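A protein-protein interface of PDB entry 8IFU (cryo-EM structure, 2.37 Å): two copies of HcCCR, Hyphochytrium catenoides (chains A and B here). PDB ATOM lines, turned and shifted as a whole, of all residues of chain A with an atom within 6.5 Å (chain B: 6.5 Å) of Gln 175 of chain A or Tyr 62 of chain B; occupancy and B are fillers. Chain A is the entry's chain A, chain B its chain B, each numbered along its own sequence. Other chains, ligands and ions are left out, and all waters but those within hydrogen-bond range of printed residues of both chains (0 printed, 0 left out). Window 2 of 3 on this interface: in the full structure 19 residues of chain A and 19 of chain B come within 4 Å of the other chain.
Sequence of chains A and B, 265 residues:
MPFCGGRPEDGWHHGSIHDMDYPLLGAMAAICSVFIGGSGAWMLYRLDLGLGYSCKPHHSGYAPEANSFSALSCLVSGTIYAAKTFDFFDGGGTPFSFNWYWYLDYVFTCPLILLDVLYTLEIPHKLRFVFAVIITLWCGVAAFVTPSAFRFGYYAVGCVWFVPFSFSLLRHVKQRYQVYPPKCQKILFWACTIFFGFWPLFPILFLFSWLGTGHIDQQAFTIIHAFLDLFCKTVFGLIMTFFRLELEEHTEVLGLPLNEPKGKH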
ATOM      1  N   GLU A 122     -30.886  25.403   3.813  1.00  0.00           N
ATOM      2  CA  GLU A 122     -29.859  25.209   2.795  1.00  0.00           C
ATOM      3  C   GLU A 122     -29.901  23.792   2.285  1.00  0.00           C
ATOM      4  O   GLU A 122     -28.941  23.050   2.396  1.00  0.00           O
ATOM      5  CB  GLU A 122     -28.475  25.618   3.303  1.00  0.00           C
ATOM      6  CG  GLU A 122     -28.256  27.114   3.401  1.00  0.00           C
ATOM      7  CD  GLU A 122     -28.684  27.689   4.735  1.00  0.00           C
ATOM      8  OE1 GLU A 122     -28.576  26.982   5.757  1.00  0.00           O
ATOM      9  OE2 GLU A 122     -29.136  28.853   4.759  1.00  0.00           O
ATOM     10  N   PRO A 124     -30.023  20.867  -0.663  1.00  0.00           N
ATOM     11  CA  PRO A 124     -29.749  20.662  -2.081  1.00  0.00           C
ATOM     12  C   PRO A 124     -30.938  20.214  -2.911  1.00  0.00           C
ATOM     13  O   PRO A 124     -31.976  19.910  -2.341  1.00  0.00           O
ATOM     14  CB  PRO A 124     -28.715  19.554  -2.053  1.00  0.00           C
ATOM     15  CG  PRO A 124     -28.961  18.823  -0.789  1.00  0.00           C
ATOM     16  CD  PRO A 124     -29.289  19.907   0.178  1.00  0.00           C
ATOM     17  N   HIS A 125     -30.796  20.164  -4.229  1.00  0.00           N
ATOM     18  CA  HIS A 125     -31.850  19.700  -5.138  1.00  0.00           C
ATOM     19  C   HIS A 125     -33.128  20.467  -5.045  1.00  0.00           C
ATOM     20  O   HIS A 125     -34.187  19.895  -5.141  1.00  0.00           O
ATOM     21  CB  HIS A 125     -32.118  18.203  -5.015  1.00  0.00           C
ATOM     22  CG  HIS A 125     -30.891  17.375  -4.818  1.00  0.00           C
ATOM     23  ND1 HIS A 125     -29.757  17.523  -5.585  1.00  0.00           N
ATOM     24  CD2 HIS A 125     -30.626  16.380  -3.942  1.00  0.00           C
ATOM     25  CE1 HIS A 125     -28.843  16.661  -5.184  1.00  0.00           C
ATOM     26  NE2 HIS A 125     -29.346  15.954  -4.189  1.00  0.00           N
ATOM     27  N   ARG A 128     -35.520  19.901  -8.052  1.00  0.00           N
ATOM     28  CA  ARG A 128     -36.116  18.596  -8.030  1.00  0.00           C
ATOM     29  C   ARG A 128     -37.222  18.517  -7.029  1.00  0.00           C
ATOM     30  O   ARG A 128     -38.243  17.920  -7.297  1.00  0.00           O
ATOM     31  CB  ARG A 128     -35.065  17.575  -7.659  1.00  0.00           C
ATOM     32  CG  ARG A 128     -33.895  17.458  -8.600  1.00  0.00           C
ATOM     33  CD  ARG A 128     -33.214  16.140  -8.313  1.00  0.00           C
ATOM     34  NE  ARG A 128     -31.791  16.155  -8.599  1.00  0.00           N
ATOM     35  CZ  ARG A 128     -30.943  15.255  -8.125  1.00  0.00           C
ATOM     36  NH1 ARG A 128     -31.385  14.289  -7.338  1.00  0.00           N
ATOM     37  NH2 ARG A 128     -29.660  15.323  -8.433  1.00  0.00           N
ATOM     38  N   SER A 168     -36.523  11.683   0.752  1.00  0.00           N
ATOM     39  CA  SER A 168     -35.322  12.380   0.401  1.00  0.00           C
ATOM     40  C   SER A 168     -35.191  13.662   1.186  1.00  0.00           C
ATOM     41  O   SER A 168     -34.105  14.013   1.599  1.00  0.00           O
ATOM     42  CB  SER A 168     -35.304  12.645  -1.093  1.00  0.00           C
ATOM     43  OG  SER A 168     -33.997  12.947  -1.530  1.00  0.00           O
ATOM     44  N   LEU A 170     -36.629  14.240   4.200  1.00  0.00           N
ATOM     45  CA  LEU A 170     -36.344  13.899   5.568  1.00  0.00           C
ATOM     46  C   LEU A 170     -34.874  13.592   5.775  1.00  0.00           C
ATOM     47  O   LEU A 170     -34.311  13.975   6.778  1.00  0.00           O
ATOM     48  CB  LEU A 170     -37.230  12.752   6.029  1.00  0.00           C
ATOM     49  CG  LEU A 170     -37.612  12.531   7.490  1.00  0.00           C
ATOM     50  CD1 LEU A 170     -37.510  13.790   8.330  1.00  0.00           C
ATOM     51  CD2 LEU A 170     -39.020  11.974   7.549  1.00  0.00           C
ATOM     52  N   ARG A 171     -34.235  12.928   4.835  1.00  0.00           N
ATOM     53  CA  ARG A 171     -32.831  12.635   4.943  1.00  0.00           C
ATOM     54  C   ARG A 171     -32.029  13.894   4.951  1.00  0.00           C
ATOM     55  O   ARG A 171     -31.139  14.051   5.765  1.00  0.00           O
ATOM     56  CB  ARG A 171     -32.401  11.791   3.768  1.00  0.00           C
ATOM     57  CG  ARG A 171     -31.957  10.390   4.122  1.00  0.00           C
ATOM     58  CD  ARG A 171     -31.447   9.674   2.885  1.00  0.00           C
ATOM     59  NE  ARG A 171     -32.535   9.165   2.056  1.00  0.00           N
ATOM     60  CZ  ARG A 171     -32.796   9.583   0.821  1.00  0.00           C
ATOM     61  NH1 ARG A 171     -32.047  10.527   0.265  1.00  0.00           N
ATOM     62  NH2 ARG A 171     -33.809   9.059   0.146  1.00  0.00           N
ATOM     63  N   HIS A 172     -32.343  14.803   4.050  1.00  0.00           N
ATOM     64  CA  HIS A 172     -31.655  16.064   3.975  1.00  0.00           C
ATOM     65  C   HIS A 172     -31.854  16.956   5.169  1.00  0.00           C
ATOM     66  O   HIS A 172     -30.921  17.591   5.606  1.00  0.00           O
ATOM     67  CB  HIS A 172     -32.092  16.792   2.730  1.00  0.00           C
ATOM     68  CG  HIS A 172     -31.490  16.255   1.474  1.00  0.00           C
ATOM     69  ND1 HIS A 172     -30.196  15.790   1.408  1.00  0.00           N
ATOM     70  CD2 HIS A 172     -32.005  16.110   0.231  1.00  0.00           C
ATOM     71  CE1 HIS A 172     -29.942  15.377   0.181  1.00  0.00           C
ATOM     72  NE2 HIS A 172     -31.023  15.559  -0.553  1.00  0.00           N
ATOM     73  N   VAL A 173     -33.054  17.009   5.712  1.00  0.00           N
ATOM     74  CA  VAL A 173     -33.295  17.800   6.899  1.00  0.00           C
ATOM     75  C   VAL A 173     -32.711  17.210   8.166  1.00  0.00           C
ATOM     76  O   VAL A 173     -32.474  17.928   9.110  1.00  0.00           O
ATOM     77  CB  VAL A 173     -34.771  18.193   7.096  1.00  0.00           C
ATOM     78  CG1 VAL A 173     -35.362  18.802   5.844  1.00  0.00           C
ATOM     79  CG2 VAL A 173     -35.594  17.056   7.653  1.00  0.00           C
ATOM     80  N   LYS A 174     -32.445  15.920   8.183  1.00  0.00           N
ATOM     81  CA  LYS A 174     -31.829  15.316   9.331  1.00  0.00           C
ATOM     82  C   LYS A 174     -30.363  15.615   9.303  1.00  0.00           C
ATOM     83  O   LYS A 174     -29.741  15.784  10.342  1.00  0.00           O
ATOM     84  CB  LYS A 174     -32.060  13.827   9.325  1.00  0.00           C
ATOM     85  CG  LYS A 174     -33.334  13.382  10.011  1.00  0.00           C
ATOM     86  CD  LYS A 174     -33.361  11.871  10.143  1.00  0.00           C
ATOM     87  CE  LYS A 174     -34.012  11.223   8.933  1.00  0.00           C
ATOM     88  NZ  LYS A 174     -33.021  10.586   8.021  1.00  0.00           N
ATOM     89  N   GLN A 175     -29.803  15.721   8.116  1.00  0.00           N
ATOM     90  CA  GLN A 175     -28.410  16.080   7.992  1.00  0.00           C
ATOM     91  C   GLN A 175     -28.194  17.507   8.432  1.00  0.00           C
ATOM     92  O   GLN A 175     -27.222  17.805   9.110  1.00  0.00           O
ATOM     93  CB  GLN A 175     -27.953  15.921   6.548  1.00  0.00           C
ATOM     94  CG  GLN A 175     -27.817  14.491   6.070  1.00  0.00           C
ATOM     95  CD  GLN A 175     -28.014  14.376   4.574  1.00  0.00           C
ATOM     96  OE1 GLN A 175     -27.789  15.334   3.837  1.00  0.00           O
ATOM     97  NE2 GLN A 175     -28.443  13.208   4.116  1.00  0.00           N
ATOM     98  N   ARG A 176     -29.102  18.391   8.059  1.00  0.00           N
ATOM     99  CA  ARG A 176     -28.990  19.776   8.427  1.00  0.00           C
ATOM    100  C   ARG A 176     -29.291  20.022   9.891  1.00  0.00           C
ATOM    101  O   ARG A 176     -28.707  20.895  10.491  1.00  0.00           O
ATOM    102  CB  ARG A 176     -29.888  20.610   7.530  1.00  0.00           C
ATOM    103  CG  ARG A 176     -29.436  20.655   6.087  1.00  0.00           C
ATOM    104  CD  ARG A 176     -28.066  21.293   5.967  1.00  0.00           C
ATOM    105  NE  ARG A 176     -28.080  22.680   6.417  1.00  0.00           N
ATOM    106  CZ  ARG A 176     -26.992  23.399   6.649  1.00  0.00           C
ATOM    107  NH1 ARG A 176     -25.798  22.863   6.478  1.00  0.00           N
ATOM    108  NH2 ARG A 176     -27.100  24.651   7.055  1.00  0.00           N
ATOM    109  N   TYR A 177     -30.173  19.241  10.486  1.00  0.00           N
ATOM    110  CA  TYR A 177     -30.532  19.398  11.878  1.00  0.00           C
ATOM    111  C   TYR A 177     -29.329  19.440  12.793  1.00  0.00           C
ATOM    112  O   TYR A 177     -29.297  20.222  13.721  1.00  0.00           O
ATOM    113  CB  TYR A 177     -31.466  18.269  12.269  1.00  0.00           C
ATOM    114  CG  TYR A 177     -32.293  18.417  13.518  1.00  0.00           C
ATOM    115  CD1 TYR A 177     -33.560  18.971  13.469  1.00  0.00           C
ATOM    116  CD2 TYR A 177     -31.842  17.924  14.730  1.00  0.00           C
ATOM    117  CE1 TYR A 177     -34.334  19.077  14.604  1.00  0.00           C
ATOM    118  CE2 TYR A 177     -32.606  18.028  15.867  1.00  0.00           C
ATOM    119  CZ  TYR A 177     -33.850  18.603  15.797  1.00  0.00           C
ATOM    120  OH  TYR A 177     -34.611  18.699  16.935  1.00  0.00           O
ATOM    121  N   GLN A 178     -28.325  18.626  12.535  1.00  0.00           N
ATOM    122  CA  GLN A 178     -27.156  18.556  13.403  1.00  0.00           C
ATOM    123  C   GLN A 178     -26.204  19.732  13.321  1.00  0.00           C
ATOM    124  O   GLN A 178     -25.339  19.883  14.170  1.00  0.00           O
ATOM    125  CB  GLN A 178     -26.407  17.277  13.110  1.00  0.00           C
ATOM    126  CG  GLN A 178     -27.272  16.035  13.176  1.00  0.00           C
ATOM    127  CD  GLN A 178     -27.080  15.142  11.971  1.00  0.00           C
ATOM    128  OE1 GLN A 178     -26.291  15.448  11.079  1.00  0.00           O
ATOM    129  NE2 GLN A 178     -27.808  14.034  11.933  1.00  0.00           N
ATOM    130  N   VAL A 179     -26.355  20.570  12.314  1.00  0.00           N
ATOM    131  CA  VAL A 179     -25.525  21.735  12.149  1.00  0.00           C
ATOM    132  C   VAL A 179     -26.028  22.804  13.067  1.00  0.00           C
ATOM    133  O   VAL A 179     -25.262  23.611  13.555  1.00  0.00           O
ATOM    134  CB  VAL A 179     -25.630  22.213  10.686  1.00  0.00           C
ATOM    135  CG1 VAL A 179     -24.646  23.316  10.383  1.00  0.00           C
ATOM    136  CG2 VAL A 179     -25.373  21.046   9.752  1.00  0.00           C
ATOM    137  N   GLU A 260     -21.213  22.661  11.801  1.00  0.00           N
ATOM    138  CA  GLU A 260     -21.050  21.931  10.537  1.00  0.00           C
ATOM    139  C   GLU A 260     -21.574  20.493  10.484  1.00  0.00           C
ATOM    140  O   GLU A 260     -21.345  19.766   9.512  1.00  0.00           O
ATOM    141  CB  GLU A 260     -19.582  21.954  10.103  1.00  0.00           C
ATOM    142  CG  GLU A 260     -18.667  22.760  11.011  1.00  0.00           C
ATOM    143  CD  GLU A 260     -17.751  21.883  11.842  1.00  0.00           C
ATOM    144  OE1 GLU A 260     -16.550  21.801  11.511  1.00  0.00           O
ATOM    145  OE2 GLU A 260     -18.230  21.276  12.824  1.00  0.00           O
ATOM    146  N   ASP B  48     -26.558  11.768  -9.505  1.00  0.00           N
ATOM    147  CA  ASP B  48     -26.099  11.707  -8.143  1.00  0.00           C
ATOM    148  C   ASP B  48     -24.951  10.761  -7.888  1.00  0.00           C
ATOM    149  O   ASP B  48     -24.338  10.821  -6.835  1.00  0.00           O
ATOM    150  CB  ASP B  48     -27.276  11.302  -7.290  1.00  0.00           C
ATOM    151  CG  ASP B  48     -28.436  12.258  -7.406  1.00  0.00           C
ATOM    152  OD1 ASP B  48     -28.196  13.474  -7.554  1.00  0.00           O
ATOM    153  OD2 ASP B  48     -29.590  11.793  -7.349  1.00  0.00           O
ATOM    154  N   HIS B  58     -18.885  14.745  -6.492  1.00  0.00           N
ATOM    155  CA  HIS B  58     -19.220  16.130  -6.809  1.00  0.00           C
ATOM    156  C   HIS B  58     -18.563  17.101  -5.863  1.00  0.00           C
ATOM    157  O   HIS B  58     -18.324  16.780  -4.707  1.00  0.00           O
ATOM    158  CB  HIS B  58     -20.717  16.339  -6.736  1.00  0.00           C
ATOM    159  CG  HIS B  58     -21.484  15.709  -7.852  1.00  0.00           C
ATOM    160  ND1 HIS B  58     -21.481  16.212  -9.133  1.00  0.00           N
ATOM    161  CD2 HIS B  58     -22.303  14.633  -7.872  1.00  0.00           C
ATOM    162  CE1 HIS B  58     -22.252  15.463  -9.899  1.00  0.00           C
ATOM    163  NE2 HIS B  58     -22.763  14.499  -9.157  1.00  0.00           N
ATOM    164  N   HIS B  59     -18.301  18.307  -6.329  1.00  0.00           N
ATOM    165  CA  HIS B  59     -17.604  19.306  -5.519  1.00  0.00           C
ATOM    166  C   HIS B  59     -18.312  19.733  -4.261  1.00  0.00           C
ATOM    167  O   HIS B  59     -17.707  19.787  -3.197  1.00  0.00           O
ATOM    168  CB  HIS B  59     -17.329  20.532  -6.372  1.00  0.00           C
ATOM    169  CG  HIS B  59     -16.750  20.209  -7.715  1.00  0.00           C
ATOM    170  ND1 HIS B  59     -15.610  19.452  -7.868  1.00  0.00           N
ATOM    171  CD2 HIS B  59     -17.159  20.533  -8.963  1.00  0.00           C
ATOM    172  CE1 HIS B  59     -15.338  19.328  -9.154  1.00  0.00           C
ATOM    173  NE2 HIS B  59     -16.263  19.975  -9.839  1.00  0.00           N
ATOM    174  N   SER B  60     -19.594  20.040  -4.368  1.00  0.00           N
ATOM    175  CA  SER B  60     -20.367  20.443  -3.211  1.00  0.00           C
ATOM    176  C   SER B  60     -20.920  19.236  -2.490  1.00  0.00           C
ATOM    177  O   SER B  60     -21.469  19.361  -1.403  1.00  0.00           O
ATOM    178  CB  SER B  60     -21.500  21.355  -3.651  1.00  0.00           C
ATOM    179  OG  SER B  60     -22.616  20.601  -4.079  1.00  0.00           O
ATOM    180  N   GLY B  61     -20.781  18.064  -3.082  1.00  0.00           N
ATOM    181  CA  GLY B  61     -21.295  16.853  -2.492  1.00  0.00           C
ATOM    182  C   GLY B  61     -22.556  16.504  -3.206  1.00  0.00           C
ATOM    183  O   GLY B  61     -23.008  15.372  -3.143  1.00  0.00           O
ATOM    184  N   TYR B  62     -23.132  17.477  -3.891  1.00  0.00           N
ATOM    185  CA  TYR B  62     -24.379  17.272  -4.589  1.00  0.00           C
ATOM    186  C   TYR B  62     -24.241  17.715  -6.007  1.00  0.00           C
ATOM    187  O   TYR B  62     -23.357  18.490  -6.334  1.00  0.00           O
ATOM    188  CB  TYR B  62     -25.509  18.036  -3.909  1.00  0.00           C
ATOM    189  CG  TYR B  62     -25.570  17.809  -2.426  1.00  0.00           C
ATOM    190  CD1 TYR B  62     -26.097  16.636  -1.910  1.00  0.00           C
ATOM    191  CD2 TYR B  62     -25.082  18.754  -1.538  1.00  0.00           C
ATOM    192  CE1 TYR B  62     -26.141  16.414  -0.552  1.00  0.00           C
ATOM    193  CE2 TYR B  62     -25.120  18.539  -0.179  1.00  0.00           C
ATOM    194  CZ  TYR B  62     -25.652  17.368   0.304  1.00  0.00           C
ATOM    195  OH  TYR B  62     -25.699  17.152   1.658  1.00  0.00           O
ATOM    196  N   ALA B  63     -25.128  17.237  -6.859  1.00  0.00           N
ATOM    197  CA  ALA B  63     -25.062  17.556  -8.268  1.00  0.00           C
ATOM    198  C   ALA B  63     -25.459  18.970  -8.532  1.00  0.00           C
ATOM    199  O   ALA B  63     -26.314  19.497  -7.847  1.00  0.00           O
ATOM    200  CB  ALA B  63     -25.955  16.602  -9.041  1.00  0.00           C
ATOM    201  N   PRO B  64     -24.837  19.604  -9.534  1.00  0.00           N
ATOM    202  CA  PRO B  64     -25.269  20.954  -9.902  1.00  0.00           C
ATOM    203  C   PRO B  64     -26.738  20.980 -10.268  1.00  0.00           C
ATOM    204  O   PRO B  64     -27.223  20.054 -10.904  1.00  0.00           O
ATOM    205  CB  PRO B  64     -24.392  21.277 -11.092  1.00  0.00           C
ATOM    206  CG  PRO B  64     -23.148  20.505 -10.847  1.00  0.00           C
ATOM    207  CD  PRO B  64     -23.595  19.219 -10.223  1.00  0.00           C
ATOM    208  N   GLU B  65     -27.451  22.027  -9.887  1.00  0.00           N
ATOM    209  CA  GLU B  65     -28.888  22.079 -10.103  1.00  0.00           C
ATOM    210  C   GLU B  65     -29.362  22.112 -11.519  1.00  0.00           C
ATOM    211  O   GLU B  65     -30.479  21.710 -11.804  1.00  0.00           O
ATOM    212  CB  GLU B  65     -29.460  23.269  -9.364  1.00  0.00           C
ATOM    213  CG  GLU B  65     -30.471  22.891  -8.294  1.00  0.00           C
ATOM    214  CD  GLU B  65     -29.985  23.190  -6.891  1.00  0.00           C
ATOM    215  OE1 GLU B  65     -30.283  24.285  -6.378  1.00  0.00           O
ATOM    216  OE2 GLU B  65     -29.307  22.328  -6.295  1.00  0.00           O
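N of His 125 of chain A is in hydrogen-bond range of OE2 of Glu 65 of chain B.
NH2 of Arg 128 of chain A is in salt-bridge range of OD1 of Asp 48 of chain B.
ND1 of His 172 of chain A is in hydrogen-bond range of OE1 of Gln 175 of chain A, 3.4 Å away.
The backbone carbonyl oxygen (O) of Arg 171 of chain A is in hydrogen-bond range of the side-chain amide nitrogen (NE2) of Gln 175 of chain A (3.3 Å).
The backbone NH (N) of Tyr 62 of chain B lies close to the side-chain hydroxyl (OG) of Ser 60 of chain B, 3.2 Å away.
O of Gln 175 of chain A sits close to OE1 of Gln 178 of chain A, at 3.2 Å.
CG of Tyr 62 of chain B touches CB of Pro 124 of chain A, at 3.6 Å.
His 125 of chain A touches Tyr 62 of chain B.
CB of Ala 63 of chain B touches NH2 of Arg 128 of chain A, at 3.97 Å.
Tyr 62 of chain B touches Gln 175 of chain A (OH to OE1, 3.5 Å).
Of chain B, only Tyr 62 (3.5 Å) comes within 4 Å of Gln 175 of chain A.
Of the printed residues of chain A, Tyr 62 of chain B touches Pro 124, His 125 and Gln 175.
Of the printed residues of chain A, Ala 63 of chain B touches Arg 128 (3.97 Å).
Of the printed residues of chain B, Arg 128 of chain A touches Asp 48 (2.5 Å) and Ala 63 (3.97 Å).
Printed residues of chain A within 4 Å of Asp 48 of chain B: Arg 128 (2.5 Å).
Printed residues of chain A that touch a printed residue of chain B: Pro 124, His 125, Arg 128 and Gln 175.
Hydrophobic or aromatic side chains of chain B that line the printed part of chain A: Tyr 62 and Ala 63.
Along chain B the printed residues that touch a printed residue of chain A span positions 48 to 65.
Among the printed residues, 6 pairs touch across the chains.
No position is printed for both chains.
Of the 6 pairs that touch across the chains among the printed residues, none has its exchanged pair printed and touching as well.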
